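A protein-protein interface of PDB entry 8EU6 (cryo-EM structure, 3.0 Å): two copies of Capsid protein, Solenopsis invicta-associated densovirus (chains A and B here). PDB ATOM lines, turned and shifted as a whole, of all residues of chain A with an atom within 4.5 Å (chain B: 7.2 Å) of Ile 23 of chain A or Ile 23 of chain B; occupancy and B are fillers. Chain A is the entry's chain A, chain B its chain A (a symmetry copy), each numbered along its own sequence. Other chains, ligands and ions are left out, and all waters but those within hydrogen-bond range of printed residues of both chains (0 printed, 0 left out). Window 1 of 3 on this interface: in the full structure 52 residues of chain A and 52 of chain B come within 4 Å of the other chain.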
ATOM      1  N   VAL A  22      -6.220 -18.919  33.524  1.00  0.00           N
ATOM      2  CA  VAL A  22      -5.724 -19.489  32.283  1.00  0.00           C
ATOM      3  C   VAL A  22      -6.865 -20.182  31.563  1.00  0.00           C
ATOM      4  O   VAL A  22      -7.810 -20.679  32.183  1.00  0.00           O
ATOM      5  CB  VAL A  22      -4.574 -20.478  32.533  1.00  0.00           C
ATOM      6  CG1 VAL A  22      -5.047 -21.629  33.382  1.00  0.00           C
ATOM      7  CG2 VAL A  22      -4.059 -20.997  31.235  1.00  0.00           C
ATOM      8  N   ILE A  23      -6.767 -20.219  30.241  1.00  0.00           N
ATOM      9  CA  ILE A  23      -7.744 -20.881  29.391  1.00  0.00           C
ATOM     10  C   ILE A  23      -6.993 -21.672  28.339  1.00  0.00           C
ATOM     11  O   ILE A  23      -6.228 -21.099  27.554  1.00  0.00           O
ATOM     12  CB  ILE A  23      -8.697 -19.878  28.734  1.00  0.00           C
ATOM     13  CG1 ILE A  23      -9.567 -19.234  29.795  1.00  0.00           C
ATOM     14  CG2 ILE A  23      -9.542 -20.570  27.715  1.00  0.00           C
ATOM     15  CD1 ILE A  23     -10.355 -18.092  29.288  1.00  0.00           C
ATOM     16  N   ARG A  24      -7.218 -22.975  28.311  1.00  0.00           N
ATOM     17  CA  ARG A  24      -6.562 -23.856  27.358  1.00  0.00           C
ATOM     18  C   ARG A  24      -7.511 -24.088  26.194  1.00  0.00           C
ATOM     19  O   ARG A  24      -8.561 -24.718  26.353  1.00  0.00           O
ATOM     20  CB  ARG A  24      -6.157 -25.172  28.012  1.00  0.00           C
ATOM     21  CG  ARG A  24      -5.473 -26.121  27.058  1.00  0.00           C
ATOM     22  CD  ARG A  24      -5.080 -27.414  27.722  1.00  0.00           C
ATOM     23  NE  ARG A  24      -4.043 -27.209  28.724  1.00  0.00           N
ATOM     24  CZ  ARG A  24      -3.532 -28.180  29.473  1.00  0.00           C
ATOM     25  NH1 ARG A  24      -3.959 -29.428  29.335  1.00  0.00           N
ATOM     26  NH2 ARG A  24      -2.589 -27.901  30.359  1.00  0.00           N
ATOM     27  N   ASN A  25      -7.141 -23.572  25.031  1.00  0.00           N
ATOM     28  CA  ASN A  25      -7.869 -23.806  23.798  1.00  0.00           C
ATOM     29  C   ASN A  25      -6.991 -24.592  22.845  1.00  0.00           C
ATOM     30  O   ASN A  25      -5.771 -24.414  22.818  1.00  0.00           O
ATOM     31  CB  ASN A  25      -8.284 -22.510  23.133  1.00  0.00           C
ATOM     32  CG  ASN A  25      -9.258 -22.729  22.008  1.00  0.00           C
ATOM     33  OD1 ASN A  25     -10.081 -23.639  22.051  1.00  0.00           O
ATOM     34  ND2 ASN A  25      -9.152 -21.914  20.976  1.00  0.00           N
ATOM     35  N   LEU A  77     -10.237 -15.014  22.549  1.00  0.00           N
ATOM     36  CA  LEU A  77      -9.376 -15.191  23.709  1.00  0.00           C
ATOM     37  C   LEU A  77      -8.124 -14.337  23.608  1.00  0.00           C
ATOM     38  O   LEU A  77      -7.543 -13.964  24.632  1.00  0.00           O
ATOM     39  CB  LEU A  77      -9.010 -16.661  23.860  1.00  0.00           C
ATOM     40  CG  LEU A  77     -10.016 -17.515  24.623  1.00  0.00           C
ATOM     41  CD1 LEU A  77     -11.317 -17.571  23.905  1.00  0.00           C
ATOM     42  CD2 LEU A  77      -9.498 -18.906  24.787  1.00  0.00           C
ATOM     43  N   MET A 275      -3.201 -24.291  22.951  1.00  0.00           N
ATOM     44  CA  MET A 275      -2.872 -22.940  23.362  1.00  0.00           C
ATOM     45  C   MET A 275      -3.452 -22.692  24.740  1.00  0.00           C
ATOM     46  O   MET A 275      -4.639 -22.936  24.973  1.00  0.00           O
ATOM     47  CB  MET A 275      -3.436 -21.933  22.375  1.00  0.00           C
ATOM     48  CG  MET A 275      -2.838 -22.034  21.012  1.00  0.00           C
ATOM     49  SD  MET A 275      -3.676 -21.012  19.807  1.00  0.00           S
ATOM     50  CE  MET A 275      -3.233 -19.406  20.413  1.00  0.00           C
ATOM     51  N   GLU A 276      -2.620 -22.215  25.652  1.00  0.00           N
ATOM     52  CA  GLU A 276      -3.068 -21.838  26.983  1.00  0.00           C
ATOM     53  C   GLU A 276      -3.055 -20.322  27.046  1.00  0.00           C
ATOM     54  O   GLU A 276      -1.988 -19.708  27.138  1.00  0.00           O
ATOM     55  CB  GLU A 276      -2.181 -22.443  28.067  1.00  0.00           C
ATOM     56  N   HIS A 277      -4.236 -19.726  27.013  1.00  0.00           N
ATOM     57  CA  HIS A 277      -4.365 -18.286  27.090  1.00  0.00           C
ATOM     58  C   HIS A 277      -4.410 -17.868  28.545  1.00  0.00           C
ATOM     59  O   HIS A 277      -5.212 -18.390  29.325  1.00  0.00           O
ATOM     60  CB  HIS A 277      -5.625 -17.806  26.383  1.00  0.00           C
ATOM     61  CG  HIS A 277      -5.635 -18.061  24.914  1.00  0.00           C
ATOM     62  ND1 HIS A 277      -6.028 -19.263  24.370  1.00  0.00           N
ATOM     63  CD2 HIS A 277      -5.306 -17.265  23.874  1.00  0.00           C
ATOM     64  CE1 HIS A 277      -5.941 -19.195  23.056  1.00  0.00           C
ATOM     65  NE2 HIS A 277      -5.504 -17.993  22.729  1.00  0.00           N
ATOM     66  N   ILE A 279      -5.620 -15.026  30.621  1.00  0.00           N
ATOM     67  CA  ILE A 279      -6.546 -13.939  30.371  1.00  0.00           C
ATOM     68  C   ILE A 279      -6.069 -12.685  31.080  1.00  0.00           C
ATOM     69  O   ILE A 279      -5.391 -12.741  32.113  1.00  0.00           O
ATOM     70  CB  ILE A 279      -7.966 -14.314  30.818  1.00  0.00           C
ATOM     71  CG1 ILE A 279      -7.983 -14.619  32.308  1.00  0.00           C
ATOM     72  CG2 ILE A 279      -8.459 -15.496  30.046  1.00  0.00           C
ATOM     73  CD1 ILE A 279      -9.362 -14.775  32.851  1.00  0.00           C
ATOM     74  N   GLN B  21     -16.290 -28.630  25.420  1.00  0.00           N
ATOM     75  CA  GLN B  21     -15.324 -27.772  26.085  1.00  0.00           C
ATOM     76  C   GLN B  21     -16.030 -26.700  26.896  1.00  0.00           C
ATOM     77  O   GLN B  21     -17.075 -26.182  26.496  1.00  0.00           O
ATOM     78  CB  GLN B  21     -14.379 -27.126  25.077  1.00  0.00           C
ATOM     79  CG  GLN B  21     -13.329 -26.262  25.730  1.00  0.00           C
ATOM     80  CD  GLN B  21     -12.220 -25.853  24.784  1.00  0.00           C
ATOM     81  OE1 GLN B  21     -12.159 -26.307  23.643  1.00  0.00           O
ATOM     82  NE2 GLN B  21     -11.344 -24.973  25.251  1.00  0.00           N
ATOM     83  N   VAL B  22     -15.440 -26.368  28.037  1.00  0.00           N
ATOM     84  CA  VAL B  22     -16.041 -25.466  29.004  1.00  0.00           C
ATOM     85  C   VAL B  22     -14.993 -24.477  29.482  1.00  0.00           C
ATOM     86  O   VAL B  22     -13.796 -24.776  29.517  1.00  0.00           O
ATOM     87  CB  VAL B  22     -16.635 -26.228  30.199  1.00  0.00           C
ATOM     88  CG1 VAL B  22     -15.556 -26.988  30.925  1.00  0.00           C
ATOM     89  CG2 VAL B  22     -17.288 -25.274  31.138  1.00  0.00           C
ATOM     90  N   ILE B  23     -15.456 -23.293  29.857  1.00  0.00           N
ATOM     91  CA  ILE B  23     -14.603 -22.238  30.383  1.00  0.00           C
ATOM     92  C   ILE B  23     -15.296 -21.630  31.585  1.00  0.00           C
ATOM     93  O   ILE B  23     -16.409 -21.104  31.464  1.00  0.00           O
ATOM     94  CB  ILE B  23     -14.308 -21.167  29.329  1.00  0.00           C
ATOM     95  CG1 ILE B  23     -13.455 -21.761  28.226  1.00  0.00           C
ATOM     96  CG2 ILE B  23     -13.611 -20.008  29.963  1.00  0.00           C
ATOM     97  CD1 ILE B  23     -13.311 -20.870  27.057  1.00  0.00           C
ATOM     98  N   ARG B  24     -14.641 -21.683  32.732  1.00  0.00           N
ATOM     99  CA  ARG B  24     -15.187 -21.143  33.966  1.00  0.00           C
ATOM    100  C   ARG B  24     -14.606 -19.756  34.177  1.00  0.00           C
ATOM    101  O   ARG B  24     -13.404 -19.606  34.414  1.00  0.00           O
ATOM    102  CB  ARG B  24     -14.887 -22.055  35.150  1.00  0.00           C
ATOM    103  CG  ARG B  24     -15.436 -21.531  36.455  1.00  0.00           C
ATOM    104  CD  ARG B  24     -15.129 -22.446  37.610  1.00  0.00           C
ATOM    105  NE  ARG B  24     -15.827 -23.719  37.490  1.00  0.00           N
ATOM    106  CZ  ARG B  24     -15.714 -24.714  38.362  1.00  0.00           C
ATOM    107  NH1 ARG B  24     -14.932 -24.587  39.425  1.00  0.00           N
ATOM    108  NH2 ARG B  24     -16.390 -25.837  38.171  1.00  0.00           N
ATOM    109  N   ASN B  25     -15.460 -18.746  34.082  1.00  0.00           N
ATOM    110  CA  ASN B  25     -15.093 -17.373  34.377  1.00  0.00           C
ATOM    111  C   ASN B  25     -15.871 -16.901  35.587  1.00  0.00           C
ATOM    112  O   ASN B  25     -17.025 -17.289  35.788  1.00  0.00           O
ATOM    113  CB  ASN B  25     -15.381 -16.451  33.211  1.00  0.00           C
ATOM    114  CG  ASN B  25     -14.770 -15.089  33.394  1.00  0.00           C
ATOM    115  OD1 ASN B  25     -13.704 -14.947  33.984  1.00  0.00           O
ATOM    116  ND2 ASN B  25     -15.458 -14.070  32.914  1.00  0.00           N
ATOM    117  N   ILE B  26     -15.236 -16.055  36.382  1.00  0.00           N
ATOM    118  CA  ILE B  26     -15.844 -15.480  37.569  1.00  0.00           C
ATOM    119  C   ILE B  26     -16.063 -14.006  37.300  1.00  0.00           C
ATOM    120  O   ILE B  26     -15.101 -13.268  37.066  1.00  0.00           O
ATOM    121  CB  ILE B  26     -14.954 -15.679  38.802  1.00  0.00           C
ATOM    122  CG1 ILE B  26     -14.736 -17.162  39.058  1.00  0.00           C
ATOM    123  CG2 ILE B  26     -15.581 -15.049  40.004  1.00  0.00           C
ATOM    124  CD1 ILE B  26     -13.791 -17.454  40.194  1.00  0.00           C
ATOM    125  N   ASN B  73     -14.409 -10.041  29.529  1.00  0.00           N
ATOM    126  CA  ASN B  73     -14.178 -11.428  29.161  1.00  0.00           C
ATOM    127  C   ASN B  73     -15.495 -12.120  28.858  1.00  0.00           C
ATOM    128  O   ASN B  73     -15.658 -12.748  27.807  1.00  0.00           O
ATOM    129  CB  ASN B  73     -13.459 -12.166  30.285  1.00  0.00           C
ATOM    130  CG  ASN B  73     -12.124 -11.563  30.618  1.00  0.00           C
ATOM    131  OD1 ASN B  73     -11.557 -10.804  29.838  1.00  0.00           O
ATOM    132  ND2 ASN B  73     -11.598 -11.922  31.775  1.00  0.00           N
ATOM    133  N   LEU B  77     -16.493 -14.292  25.832  1.00  0.00           N
ATOM    134  CA  LEU B  77     -16.852 -15.694  25.975  1.00  0.00           C
ATOM    135  C   LEU B  77     -18.297 -15.941  25.576  1.00  0.00           C
ATOM    136  O   LEU B  77     -18.644 -17.050  25.159  1.00  0.00           O
ATOM    137  CB  LEU B  77     -16.609 -16.145  27.408  1.00  0.00           C
ATOM    138  CG  LEU B  77     -15.187 -16.598  27.723  1.00  0.00           C
ATOM    139  CD1 LEU B  77     -14.225 -15.477  27.563  1.00  0.00           C
ATOM    140  CD2 LEU B  77     -15.104 -17.106  29.126  1.00  0.00           C
ATOM    141  N   ILE B  80     -18.443 -16.697  21.799  1.00  0.00           N
ATOM    142  CA  ILE B  80     -17.952 -17.994  21.374  1.00  0.00           C
ATOM    143  C   ILE B  80     -18.650 -19.137  22.076  1.00  0.00           C
ATOM    144  O   ILE B  80     -18.309 -20.301  21.833  1.00  0.00           O
ATOM    145  CB  ILE B  80     -16.437 -18.078  21.597  1.00  0.00           C
ATOM    146  CG1 ILE B  80     -16.122 -18.014  23.081  1.00  0.00           C
ATOM    147  CG2 ILE B  80     -15.778 -16.933  20.903  1.00  0.00           C
ATOM    148  CD1 ILE B  80     -14.682 -18.198  23.392  1.00  0.00           C
ATOM    149  N   VAL B  84     -24.294 -21.036  28.785  1.00  0.00           N
ATOM    150  CA  VAL B  84     -23.595 -20.882  30.050  1.00  0.00           C
ATOM    151  C   VAL B  84     -24.521 -21.322  31.171  1.00  0.00           C
ATOM    152  O   VAL B  84     -25.746 -21.256  31.056  1.00  0.00           O
ATOM    153  CB  VAL B  84     -23.137 -19.431  30.268  1.00  0.00           C
ATOM    154  CG1 VAL B  84     -24.301 -18.511  30.203  1.00  0.00           C
ATOM    155  CG2 VAL B  84     -22.480 -19.290  31.601  1.00  0.00           C
ATOM    156  N   MET B 275     -19.309 -18.312  36.396  1.00  0.00           N
ATOM    157  CA  MET B 275     -19.962 -18.644  35.145  1.00  0.00           C
ATOM    158  C   MET B 275     -19.131 -19.683  34.420  1.00  0.00           C
ATOM    159  O   MET B 275     -17.923 -19.506  34.242  1.00  0.00           O
ATOM    160  CB  MET B 275     -20.111 -17.405  34.280  1.00  0.00           C
ATOM    161  CG  MET B 275     -21.006 -16.369  34.871  1.00  0.00           C
ATOM    162  SD  MET B 275     -20.981 -14.828  33.963  1.00  0.00           S
ATOM    163  CE  MET B 275     -21.768 -15.348  32.462  1.00  0.00           C
ATOM    164  N   GLU B 276     -19.771 -20.766  34.007  1.00  0.00           N
ATOM    165  CA  GLU B 276     -19.118 -21.792  33.212  1.00  0.00           C
ATOM    166  C   GLU B 276     -19.651 -21.669  31.797  1.00  0.00           C
ATOM    167  O   GLU B 276     -20.788 -22.058  31.519  1.00  0.00           O
ATOM    168  CB  GLU B 276     -19.369 -23.187  33.777  1.00  0.00           C
ATOM    169  N   HIS B 277     -18.825 -21.143  30.906  1.00  0.00           N
ATOM    170  CA  HIS B 277     -19.201 -20.991  29.516  1.00  0.00           C
ATOM    171  C   HIS B 277     -18.883 -22.272  28.771  1.00  0.00           C
ATOM    172  O   HIS B 277     -17.755 -22.773  28.835  1.00  0.00           O
ATOM    173  CB  HIS B 277     -18.461 -19.830  28.868  1.00  0.00           C
ATOM    174  CG  HIS B 277     -18.793 -18.496  29.448  1.00  0.00           C
ATOM    175  ND1 HIS B 277     -18.176 -18.001  30.574  1.00  0.00           N
ATOM    176  CD2 HIS B 277     -19.674 -17.551  29.053  1.00  0.00           C
ATOM    177  CE1 HIS B 277     -18.664 -16.805  30.847  1.00  0.00           C
ATOM    178  NE2 HIS B 277     -19.576 -16.510  29.940  1.00  0.00           N
ATOM    179  N   HIS B 278     -19.874 -22.799  28.073  1.00  0.00           N
ATOM    180  CA  HIS B 278     -19.667 -23.911  27.164  1.00  0.00           C
ATOM    181  C   HIS B 278     -19.446 -23.324  25.780  1.00  0.00           C
ATOM    182  O   HIS B 278     -20.376 -22.795  25.166  1.00  0.00           O
ATOM    183  CB  HIS B 278     -20.866 -24.846  27.211  1.00  0.00           C
ATOM    184  CG  HIS B 278     -21.023 -25.537  28.523  1.00  0.00           C
ATOM    185  ND1 HIS B 278     -21.510 -24.900  29.642  1.00  0.00           N
ATOM    186  CD2 HIS B 278     -20.765 -26.811  28.897  1.00  0.00           C
ATOM    187  CE1 HIS B 278     -21.534 -25.748  30.652  1.00  0.00           C
ATOM    188  NE2 HIS B 278     -21.089 -26.915  30.227  1.00  0.00           N
ATOM    189  N   ILE B 279     -18.212 -23.415  25.294  1.00  0.00           N
ATOM    190  CA  ILE B 279     -17.850 -22.718  24.074  1.00  0.00           C
ATOM    191  C   ILE B 279     -18.512 -23.390  22.885  1.00  0.00           C
ATOM    192  O   ILE B 279     -18.790 -24.596  22.892  1.00  0.00           O
ATOM    193  CB  ILE B 279     -16.327 -22.673  23.898  1.00  0.00           C
ATOM    194  CG1 ILE B 279     -15.765 -24.085  23.824  1.00  0.00           C
ATOM    195  CG2 ILE B 279     -15.695 -21.928  25.031  1.00  0.00           C
ATOM    196  CD1 ILE B 279     -14.326 -24.115  23.435  1.00  0.00           C
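Of the 15 printed residues of chain B, 4 touch a printed residue of chain A. Of the 9 printed residues of chain A, 5 touch a printed residue of chain B. Printed residues of chain A that touch a printed residue of chain B: Ile 23, Arg 24, Asn 25, Leu 77 and Ile 279. Among the printed residues, 5 pairs touch across the chains.
The backbone carbonyl oxygen (O) of Arg 24 of chain A is in hydrogen-bond range of the side-chain amide nitrogen (NE2) of Gln 21 of chain B (3.0 Å).
O of Gln 21 of chain B is in hydrogen-bond range of N of Ile 279 of chain B. The backbone carbonyl oxygen of Asn 25 of chain A is in hydrogen-bond range of the backbone NH of Met 275 of chain A (2.6 Å). The backbone carbonyl oxygen (O) of Ile 23 of chain B is in hydrogen-bond range of the backbone NH (N) of His 277 of chain B. O of Ile 23 of chain A is in hydrogen-bond range of N of His 277 of chain A (2.5 Å).
Ile 23 of chain B touches its own counterpart, Ile 23 of chain A. Positions printed for both chains: 22, 23, 24, 25, 77, 275, 276, 277 and 279. Of the 5 pairs that touch across the chains among the printed residues, 1 has its exchanged pair printed and touching as well.
Among the printed residues, pairs that only touch across the chains: Leu 77 of chain A with Ile 80 of chain B (3.5 Å), Asn 25 of chain A with Gln 21 of chain B (3.7 Å), Ile 279 of chain A with Asn 73 of chain B (3.8 Å) and Ile 23 of chain A with Ile 23 of chain B (3.8 Å).
Ile 23 of chain A touches just one residue of chain B: Ile 23. Printed residues of chain B within 4 Å of Arg 24 of chain A: Gln 21. Glu 276 of chain A touches none of the printed residues of chain B. Printed residues of chain B within 4 Å of Ile 279 of chain A: Asn 73. Of the printed residues of chain A, Asn 73 of chain B touches Ile 279 (3.8 Å). The nearest printed residue of chain A that does not touch Ile 23 of chain B is Leu 77 of chain A (4.9 Å). The nearest printed residue of chain B that does not touch Leu 77 of chain A is Ile 23 of chain B (4.9 Å).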
